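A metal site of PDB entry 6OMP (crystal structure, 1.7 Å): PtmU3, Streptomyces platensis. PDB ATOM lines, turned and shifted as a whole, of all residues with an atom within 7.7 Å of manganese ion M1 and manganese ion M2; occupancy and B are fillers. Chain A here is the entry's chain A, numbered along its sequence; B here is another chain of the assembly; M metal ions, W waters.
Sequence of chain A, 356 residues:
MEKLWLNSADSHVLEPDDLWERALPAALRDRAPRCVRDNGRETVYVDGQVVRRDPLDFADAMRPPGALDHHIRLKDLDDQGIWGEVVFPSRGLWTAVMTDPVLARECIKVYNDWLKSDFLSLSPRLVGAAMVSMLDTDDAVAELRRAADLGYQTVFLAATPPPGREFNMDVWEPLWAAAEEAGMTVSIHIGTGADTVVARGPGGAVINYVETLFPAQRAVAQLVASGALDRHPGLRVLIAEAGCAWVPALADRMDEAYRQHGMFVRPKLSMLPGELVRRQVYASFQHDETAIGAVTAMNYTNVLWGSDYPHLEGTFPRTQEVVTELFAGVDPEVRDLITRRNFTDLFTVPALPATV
Manganese ion M2 is bound by OE2 of Glu 313 (2.1 Å), OD2 of Asp 308 (2.2 Å), OE2 of Glu 241 (2.2 Å), ND1 of His 311 (2.3 Å), water W1 (2.3 Å) and OE1 of Glu 241 (2.3 Å).
Within 4 Å of manganese ion M2: Glu 241, Asp 308, His 311 and Glu 313.
The backbone carbonyl oxygen of Glu 313 lies within hydrogen-bond range of the side-chain amide nitrogen of Gln 286 (2.9 Å).
OE1 of Glu 313 sits at hydrogen-bond distance from NE2 of His 261 of chain B (2.9 Å).
The backbone NH of Glu 241 lies within hydrogen-bond range of the side-chain hydroxyl of Ser 284, 3.0 Å away.
The backbone carbonyl oxygen (O) of Glu 241 sits at hydrogen-bond distance from the guanidinium group (NH1) of Arg 253 of chain B, 2.9 Å away.
The backbone carbonyl oxygen (O) of Asp 10 is in hydrogen-bond range of the backbone NH (N) of Ser 307 (3.5 Å).
The backbone carbonyl oxygen (O) of Tyr 309 sits at hydrogen-bond distance from the backbone NH (N) of His 12 (2.8 Å).
ND1 of His 12 sits at hydrogen-bond distance from O of Pro 89 (2.9 Å).
Along chain A the residues within 4 Å of manganese ion M1 span positions 10 to 308.
OD1 of Asp 308 is bound to manganese ion M1 (2.0 Å).
OE1 of Glu 241 binds manganese ion M1 (2.2 Å).
OD1 of Asp 10 binds manganese ion M1 (2.2 Å).
A ring nitrogen (NE2) of His 12 is bound to manganese ion M1.
A ring nitrogen (NE2) of His 189 is bound to manganese ion M1 (2.3 Å).
OD2 of Asp 10 is bound to manganese ion M1.
Manganese ion M1 has six donor atoms within binding distance.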
ATOM      1  N   ALA A   9      -7.203 -10.032   8.072  1.00  0.00           N
ATOM      2  CA  ALA A   9      -7.197 -10.119   6.587  1.00  0.00           C
ATOM      3  C   ALA A   9      -6.723 -11.474   6.044  1.00  0.00           C
ATOM      4  O   ALA A   9      -6.619 -11.603   4.822  1.00  0.00           O
ATOM      5  CB  ALA A   9      -6.337  -9.028   6.014  1.00  0.00           C
ATOM      6  N   ASP A  10      -6.502 -12.484   6.873  1.00  0.00           N
ATOM      7  CA  ASP A  10      -5.942 -13.759   6.409  1.00  0.00           C
ATOM      8  C   ASP A  10      -6.209 -14.895   7.401  1.00  0.00           C
ATOM      9  O   ASP A  10      -5.853 -14.826   8.572  1.00  0.00           O
ATOM     10  CB  ASP A  10      -4.442 -13.565   6.156  1.00  0.00           C
ATOM     11  CG  ASP A  10      -3.721 -14.813   5.679  1.00  0.00           C
ATOM     12  OD1 ASP A  10      -4.381 -15.721   5.187  1.00  0.00           O
ATOM     13  OD2 ASP A  10      -2.464 -14.821   5.807  1.00  0.00           O
ATOM     14  N   SER A  11      -6.785 -15.936   6.852  1.00  0.00           N
ATOM     15  CA  SER A  11      -6.923 -17.265   7.492  1.00  0.00           C
ATOM     16  C   SER A  11      -7.266 -18.271   6.425  1.00  0.00           C
ATOM     17  O   SER A  11      -7.627 -17.843   5.307  1.00  0.00           O
ATOM     18  CB  SER A  11      -7.956 -17.255   8.608  1.00  0.00           C
ATOM     19  OG  SER A  11      -9.262 -17.192   8.084  1.00  0.00           O
ATOM     20  N   HIS A  12      -7.300 -19.538   6.842  1.00  0.00           N
ATOM     21  CA  HIS A  12      -7.566 -20.658   5.915  1.00  0.00           C
ATOM     22  C   HIS A  12      -8.655 -21.561   6.500  1.00  0.00           C
ATOM     23  O   HIS A  12      -8.682 -21.774   7.733  1.00  0.00           O
ATOM     24  CB  HIS A  12      -6.303 -21.453   5.576  1.00  0.00           C
ATOM     25  CG  HIS A  12      -5.281 -20.555   4.993  1.00  0.00           C
ATOM     26  ND1 HIS A  12      -5.113 -20.409   3.629  1.00  0.00           N
ATOM     27  CD2 HIS A  12      -4.453 -19.663   5.590  1.00  0.00           C
ATOM     28  CE1 HIS A  12      -4.205 -19.453   3.428  1.00  0.00           C
ATOM     29  NE2 HIS A  12      -3.811 -18.977   4.596  1.00  0.00           N
ATOM     30  N   VAL A  86     -11.123 -12.740   6.895  1.00  0.00           N
ATOM     31  CA  VAL A  86     -11.063 -13.252   5.520  1.00  0.00           C
ATOM     32  C   VAL A  86     -10.651 -14.692   5.570  1.00  0.00           C
ATOM     33  O   VAL A  86      -9.804 -15.056   6.421  1.00  0.00           O
ATOM     34  CB  VAL A  86     -10.112 -12.399   4.658  1.00  0.00           C
ATOM     35  CG1 VAL A  86      -9.947 -12.961   3.254  1.00  0.00           C
ATOM     36  CG2 VAL A  86     -10.569 -10.960   4.616  1.00  0.00           C
ATOM     37  N   PHE A  88      -9.329 -17.883   3.248  1.00  0.00           N
ATOM     38  CA  PHE A  88      -8.746 -18.419   2.010  1.00  0.00           C
ATOM     39  C   PHE A  88      -8.897 -19.930   1.972  1.00  0.00           C
ATOM     40  O   PHE A  88      -9.045 -20.586   3.003  1.00  0.00           O
ATOM     41  CB  PHE A  88      -7.268 -18.010   1.908  1.00  0.00           C
ATOM     42  CG  PHE A  88      -7.084 -16.551   1.608  1.00  0.00           C
ATOM     43  CD1 PHE A  88      -7.285 -16.053   0.328  1.00  0.00           C
ATOM     44  CD2 PHE A  88      -6.697 -15.675   2.607  1.00  0.00           C
ATOM     45  CE1 PHE A  88      -7.122 -14.695   0.080  1.00  0.00           C
ATOM     46  CE2 PHE A  88      -6.504 -14.323   2.354  1.00  0.00           C
ATOM     47  CZ  PHE A  88      -6.711 -13.830   1.093  1.00  0.00           C
ATOM     48  N   PRO A  89      -8.770 -20.556   0.776  1.00  0.00           N
ATOM     49  CA  PRO A  89      -8.768 -22.016   0.697  1.00  0.00           C
ATOM     50  C   PRO A  89      -7.543 -22.647   1.339  1.00  0.00           C
ATOM     51  O   PRO A  89      -6.596 -21.931   1.663  1.00  0.00           O
ATOM     52  CB  PRO A  89      -8.767 -22.291  -0.810  1.00  0.00           C
ATOM     53  CG  PRO A  89      -9.107 -21.007  -1.486  1.00  0.00           C
ATOM     54  CD  PRO A  89      -8.660 -19.910  -0.537  1.00  0.00           C
ATOM     55  N   LEU A  93      -6.293 -24.297  -3.018  1.00  0.00           N
ATOM     56  CA  LEU A  93      -5.187 -23.473  -3.546  1.00  0.00           C
ATOM     57  C   LEU A  93      -4.454 -24.270  -4.623  1.00  0.00           C
ATOM     58  O   LEU A  93      -3.859 -23.627  -5.492  1.00  0.00           O
ATOM     59  CB  LEU A  93      -4.204 -23.123  -2.435  1.00  0.00           C
ATOM     60  CG  LEU A  93      -4.748 -22.286  -1.273  1.00  0.00           C
ATOM     61  CD1 LEU A  93      -3.689 -22.111  -0.191  1.00  0.00           C
ATOM     62  CD2 LEU A  93      -5.287 -20.978  -1.750  1.00  0.00           C
ATOM     63  N   HIS A 189      -2.577 -14.420  -2.678  1.00  0.00           N
ATOM     64  CA  HIS A 189      -2.034 -15.053  -1.460  1.00  0.00           C
ATOM     65  C   HIS A 189      -0.702 -15.690  -1.833  1.00  0.00           C
ATOM     66  O   HIS A 189      -0.618 -16.438  -2.838  1.00  0.00           O
ATOM     67  CB  HIS A 189      -3.012 -16.027  -0.790  1.00  0.00           C
ATOM     68  CG  HIS A 189      -2.521 -16.464   0.533  1.00  0.00           C
ATOM     69  ND1 HIS A 189      -1.417 -17.280   0.681  1.00  0.00           N
ATOM     70  CD2 HIS A 189      -3.044 -16.304   1.767  1.00  0.00           C
ATOM     71  CE1 HIS A 189      -1.190 -17.484   1.944  1.00  0.00           C
ATOM     72  NE2 HIS A 189      -2.189 -16.914   2.658  1.00  0.00           N
ATOM     73  N   ILE A 190       0.315 -15.463  -1.016  1.00  0.00           N
ATOM     74  CA  ILE A 190       1.633 -16.043  -1.388  1.00  0.00           C
ATOM     75  C   ILE A 190       1.665 -17.554  -1.193  1.00  0.00           C
ATOM     76  O   ILE A 190       0.742 -18.196  -0.575  1.00  0.00           O
ATOM     77  CB  ILE A 190       2.831 -15.338  -0.698  1.00  0.00           C
ATOM     78  CG1 ILE A 190       2.759 -15.210   0.813  1.00  0.00           C
ATOM     79  CG2 ILE A 190       3.046 -13.987  -1.364  1.00  0.00           C
ATOM     80  CD1 ILE A 190       2.716 -16.469   1.585  1.00  0.00           C
ATOM     81  N   TYR A 209      11.002 -19.746   3.431  1.00  0.00           N
ATOM     82  CA  TYR A 209      10.007 -18.788   3.944  1.00  0.00           C
ATOM     83  C   TYR A 209      10.243 -17.441   3.272  1.00  0.00           C
ATOM     84  O   TYR A 209       9.254 -16.772   2.931  1.00  0.00           O
ATOM     85  CB  TYR A 209       9.981 -18.743   5.466  1.00  0.00           C
ATOM     86  CG  TYR A 209       8.731 -18.121   6.007  1.00  0.00           C
ATOM     87  CD1 TYR A 209       7.485 -18.671   5.746  1.00  0.00           C
ATOM     88  CD2 TYR A 209       8.760 -16.967   6.771  1.00  0.00           C
ATOM     89  CE1 TYR A 209       6.321 -18.090   6.213  1.00  0.00           C
ATOM     90  CE2 TYR A 209       7.601 -16.399   7.301  1.00  0.00           C
ATOM     91  CZ  TYR A 209       6.367 -16.982   7.033  1.00  0.00           C
ATOM     92  OH  TYR A 209       5.209 -16.413   7.499  1.00  0.00           O
ATOM     93  N   ALA A 240      -1.657 -11.091   0.440  1.00  0.00           N
ATOM     94  CA  ALA A 240      -1.834 -11.788   1.732  1.00  0.00           C
ATOM     95  C   ALA A 240      -0.624 -12.633   2.126  1.00  0.00           C
ATOM     96  O   ALA A 240      -0.177 -13.497   1.328  1.00  0.00           O
ATOM     97  CB  ALA A 240      -3.112 -12.592   1.658  1.00  0.00           C
ATOM     98  N   GLU A 241      -0.131 -12.410   3.346  1.00  0.00           N
ATOM     99  CA  GLU A 241       0.789 -13.286   4.104  1.00  0.00           C
ATOM    100  C   GLU A 241       2.236 -13.090   3.611  1.00  0.00           C
ATOM    101  O   GLU A 241       3.075 -13.991   3.824  1.00  0.00           O
ATOM    102  CB  GLU A 241       0.385 -14.753   4.009  1.00  0.00           C
ATOM    103  CG  GLU A 241       0.829 -15.509   5.250  1.00  0.00           C
ATOM    104  CD  GLU A 241       0.669 -17.004   5.235  1.00  0.00           C
ATOM    105  OE1 GLU A 241      -0.464 -17.506   4.910  1.00  0.00           O
ATOM    106  OE2 GLU A 241       1.625 -17.727   5.659  1.00  0.00           O
ATOM    107  N   ALA A 242       2.511 -11.902   3.141  1.00  0.00           N
ATOM    108  CA  ALA A 242       3.887 -11.567   2.647  1.00  0.00           C
ATOM    109  C   ALA A 242       4.556 -10.535   3.552  1.00  0.00           C
ATOM    110  O   ALA A 242       5.689 -10.150   3.252  1.00  0.00           O
ATOM    111  CB  ALA A 242       3.758 -11.170   1.197  1.00  0.00           C
ATOM    112  N   SER A 284      -0.898  -7.796   4.084  1.00  0.00           N
ATOM    113  CA  SER A 284      -1.172  -8.309   5.423  1.00  0.00           C
ATOM    114  C   SER A 284       0.101  -8.856   6.070  1.00  0.00           C
ATOM    115  O   SER A 284       1.105  -9.251   5.353  1.00  0.00           O
ATOM    116  CB  SER A 284      -2.304  -9.291   5.339  1.00  0.00           C
ATOM    117  OG  SER A 284      -1.849 -10.586   4.948  1.00  0.00           O
ATOM    118  N   GLN A 286       1.343 -10.936  10.220  1.00  0.00           N
ATOM    119  CA  GLN A 286       0.883 -11.576  11.471  1.00  0.00           C
ATOM    120  C   GLN A 286       1.701 -10.989  12.625  1.00  0.00           C
ATOM    121  O   GLN A 286       1.095 -10.482  13.590  1.00  0.00           O
ATOM    122  CB  GLN A 286       0.902 -13.102  11.410  1.00  0.00           C
ATOM    123  CG  GLN A 286       0.156 -13.698  10.198  1.00  0.00           C
ATOM    124  CD  GLN A 286       1.099 -13.907   9.034  1.00  0.00           C
ATOM    125  OE1 GLN A 286       0.909 -13.316   7.977  1.00  0.00           O
ATOM    126  NE2 GLN A 286       2.079 -14.790   9.215  1.00  0.00           N
ATOM    127  N   SER A 307      -4.420 -12.985  11.152  1.00  0.00           N
ATOM    128  CA  SER A 307      -4.075 -14.024  12.125  1.00  0.00           C
ATOM    129  C   SER A 307      -3.358 -15.194  11.465  1.00  0.00           C
ATOM    130  O   SER A 307      -2.671 -15.893  12.176  1.00  0.00           O
ATOM    131  CB  SER A 307      -5.274 -14.574  12.844  1.00  0.00           C
ATOM    132  OG  SER A 307      -5.992 -15.481  12.025  1.00  0.00           O
ATOM    133  N   ASP A 308      -3.644 -15.425  10.203  1.00  0.00           N
ATOM    134  CA  ASP A 308      -3.277 -16.622   9.417  1.00  0.00           C
ATOM    135  C   ASP A 308      -3.631 -17.904  10.151  1.00  0.00           C
ATOM    136  O   ASP A 308      -3.003 -18.923   9.960  1.00  0.00           O
ATOM    137  CB  ASP A 308      -1.799 -16.660   8.975  1.00  0.00           C
ATOM    138  CG  ASP A 308      -1.568 -17.601   7.816  1.00  0.00           C
ATOM    139  OD1 ASP A 308      -2.369 -17.626   6.825  1.00  0.00           O
ATOM    140  OD2 ASP A 308      -0.472 -18.186   7.780  1.00  0.00           O
ATOM    141  N   TYR A 309      -4.736 -17.890  10.905  1.00  0.00           N
ATOM    142  CA  TYR A 309      -5.279 -19.134  11.457  1.00  0.00           C
ATOM    143  C   TYR A 309      -5.553 -20.146  10.354  1.00  0.00           C
ATOM    144  O   TYR A 309      -6.134 -19.814   9.332  1.00  0.00           O
ATOM    145  CB  TYR A 309      -6.616 -18.799  12.130  1.00  0.00           C
ATOM    146  CG  TYR A 309      -7.268 -19.928  12.900  1.00  0.00           C
ATOM    147  CD1 TYR A 309      -8.094 -20.813  12.251  1.00  0.00           C
ATOM    148  CD2 TYR A 309      -7.028 -20.104  14.260  1.00  0.00           C
ATOM    149  CE1 TYR A 309      -8.769 -21.823  12.952  1.00  0.00           C
ATOM    150  CE2 TYR A 309      -7.714 -21.074  14.980  1.00  0.00           C
ATOM    151  CZ  TYR A 309      -8.519 -21.975  14.300  1.00  0.00           C
ATOM    152  OH  TYR A 309      -9.261 -22.901  14.995  1.00  0.00           O
ATOM    153  N   PRO A 310      -5.285 -21.459  10.551  1.00  0.00           N
ATOM    154  CA  PRO A 310      -4.603 -22.035  11.694  1.00  0.00           C
ATOM    155  C   PRO A 310      -3.158 -22.446  11.459  1.00  0.00           C
ATOM    156  O   PRO A 310      -2.669 -23.382  12.125  1.00  0.00           O
ATOM    157  CB  PRO A 310      -5.356 -23.355  11.845  1.00  0.00           C
ATOM    158  CG  PRO A 310      -5.698 -23.752  10.478  1.00  0.00           C
ATOM    159  CD  PRO A 310      -5.807 -22.492   9.664  1.00  0.00           C
ATOM    160  N   HIS A 311      -2.476 -21.698  10.600  1.00  0.00           N
ATOM    161  CA  HIS A 311      -1.078 -22.017  10.206  1.00  0.00           C
ATOM    162  C   HIS A 311      -0.113 -21.769  11.402  1.00  0.00           C
ATOM    163  O   HIS A 311      -0.311 -20.824  12.216  1.00  0.00           O
ATOM    164  CB  HIS A 311      -0.727 -21.271   8.923  1.00  0.00           C
ATOM    165  CG  HIS A 311      -1.454 -21.683   7.704  1.00  0.00           C
ATOM    166  ND1 HIS A 311      -1.292 -21.007   6.510  1.00  0.00           N
ATOM    167  CD2 HIS A 311      -2.362 -22.657   7.458  1.00  0.00           C
ATOM    168  CE1 HIS A 311      -2.029 -21.577   5.587  1.00  0.00           C
ATOM    169  NE2 HIS A 311      -2.727 -22.574   6.145  1.00  0.00           N
ATOM    170  N   LEU A 312       1.031 -22.467  11.369  1.00  0.00           N
ATOM    171  CA  LEU A 312       2.113 -22.280  12.342  1.00  0.00           C
ATOM    172  C   LEU A 312       2.544 -20.811  12.349  1.00  0.00           C
ATOM    173  O   LEU A 312       2.829 -20.328  13.424  1.00  0.00           O
ATOM    174  CB  LEU A 312       3.313 -23.174  11.990  1.00  0.00           C
ATOM    175  CG  LEU A 312       3.142 -24.679  12.195  1.00  0.00           C
ATOM    176  CD1 LEU A 312       4.442 -25.376  11.829  1.00  0.00           C
ATOM    177  CD2 LEU A 312       2.799 -24.984  13.648  1.00  0.00           C
ATOM    178  N   GLU A 313       2.578 -20.146  11.192  1.00  0.00           N
ATOM    179  CA  GLU A 313       3.149 -18.777  11.070  1.00  0.00           C
ATOM    180  C   GLU A 313       2.110 -17.737  11.508  1.00  0.00           C
ATOM    181  O   GLU A 313       2.402 -16.532  11.563  1.00  0.00           O
ATOM    182  CB  GLU A 313       3.680 -18.527   9.663  1.00  0.00           C
ATOM    183  CG  GLU A 313       2.668 -18.738   8.551  1.00  0.00           C
ATOM    184  CD  GLU A 313       2.561 -20.149   7.984  1.00  0.00           C
ATOM    185  OE1 GLU A 313       3.108 -21.082   8.569  1.00  0.00           O
ATOM    186  OE2 GLU A 313       1.838 -20.319   7.006  1.00  0.00           O
ATOM    187  N   GLY A 314       0.918 -18.210  11.853  1.00  0.00           N
ATOM    188  CA  GLY A 314      -0.090 -17.299  12.413  1.00  0.00           C
ATOM    189  C   GLY A 314       0.090 -17.074  13.892  1.00  0.00           C
ATOM    190  O   GLY A 314       1.034 -17.612  14.483  1.00  0.00           O
ATOM    191  N   ARG B 253      10.655 -11.310   8.460  1.00  0.00           N
ATOM    192  CA  ARG B 253      10.221 -12.528   7.750  1.00  0.00           C
ATOM    193  C   ARG B 253      11.031 -13.705   8.328  1.00  0.00           C
ATOM    194  O   ARG B 253      10.466 -14.765   8.625  1.00  0.00           O
ATOM    195  CB  ARG B 253      10.424 -12.393   6.231  1.00  0.00           C
ATOM    196  CG  ARG B 253       9.931 -13.563   5.400  1.00  0.00           C
ATOM    197  CD  ARG B 253       8.422 -13.523   5.308  1.00  0.00           C
ATOM    198  NE  ARG B 253       7.823 -14.481   4.389  1.00  0.00           N
ATOM    199  CZ  ARG B 253       6.506 -14.648   4.334  1.00  0.00           C
ATOM    200  NH1 ARG B 253       5.732 -13.852   5.045  1.00  0.00           N
ATOM    201  NH2 ARG B 253       6.001 -15.531   3.505  1.00  0.00           N
ATOM    202  N   HIS B 261       8.402 -21.772  12.947  1.00  0.00           N
ATOM    203  CA  HIS B 261       8.744 -23.008  12.229  1.00  0.00           C
ATOM    204  C   HIS B 261      10.002 -23.656  12.833  1.00  0.00           C
ATOM    205  O   HIS B 261      10.642 -24.483  12.097  1.00  0.00           O
ATOM    206  CB  HIS B 261       8.980 -22.790  10.733  1.00  0.00           C
ATOM    207  CG  HIS B 261       7.815 -22.267   9.980  1.00  0.00           C
ATOM    208  ND1 HIS B 261       7.929 -21.819   8.697  1.00  0.00           N
ATOM    209  CD2 HIS B 261       6.521 -22.144  10.325  1.00  0.00           C
ATOM    210  CE1 HIS B 261       6.756 -21.438   8.257  1.00  0.00           C
ATOM    211  NE2 HIS B 261       5.866 -21.604   9.266  1.00  0.00           N
HETATM  212 MN    MN M   1      -2.618 -17.080   4.954  1.00  0.00          MN
HETATM  213 MN    MN M   2       0.184 -19.364   6.079  1.00  0.00          MN
HETATM  214  O   HOH W   1       0.467 -20.258   4.013  1.00  0.00           O
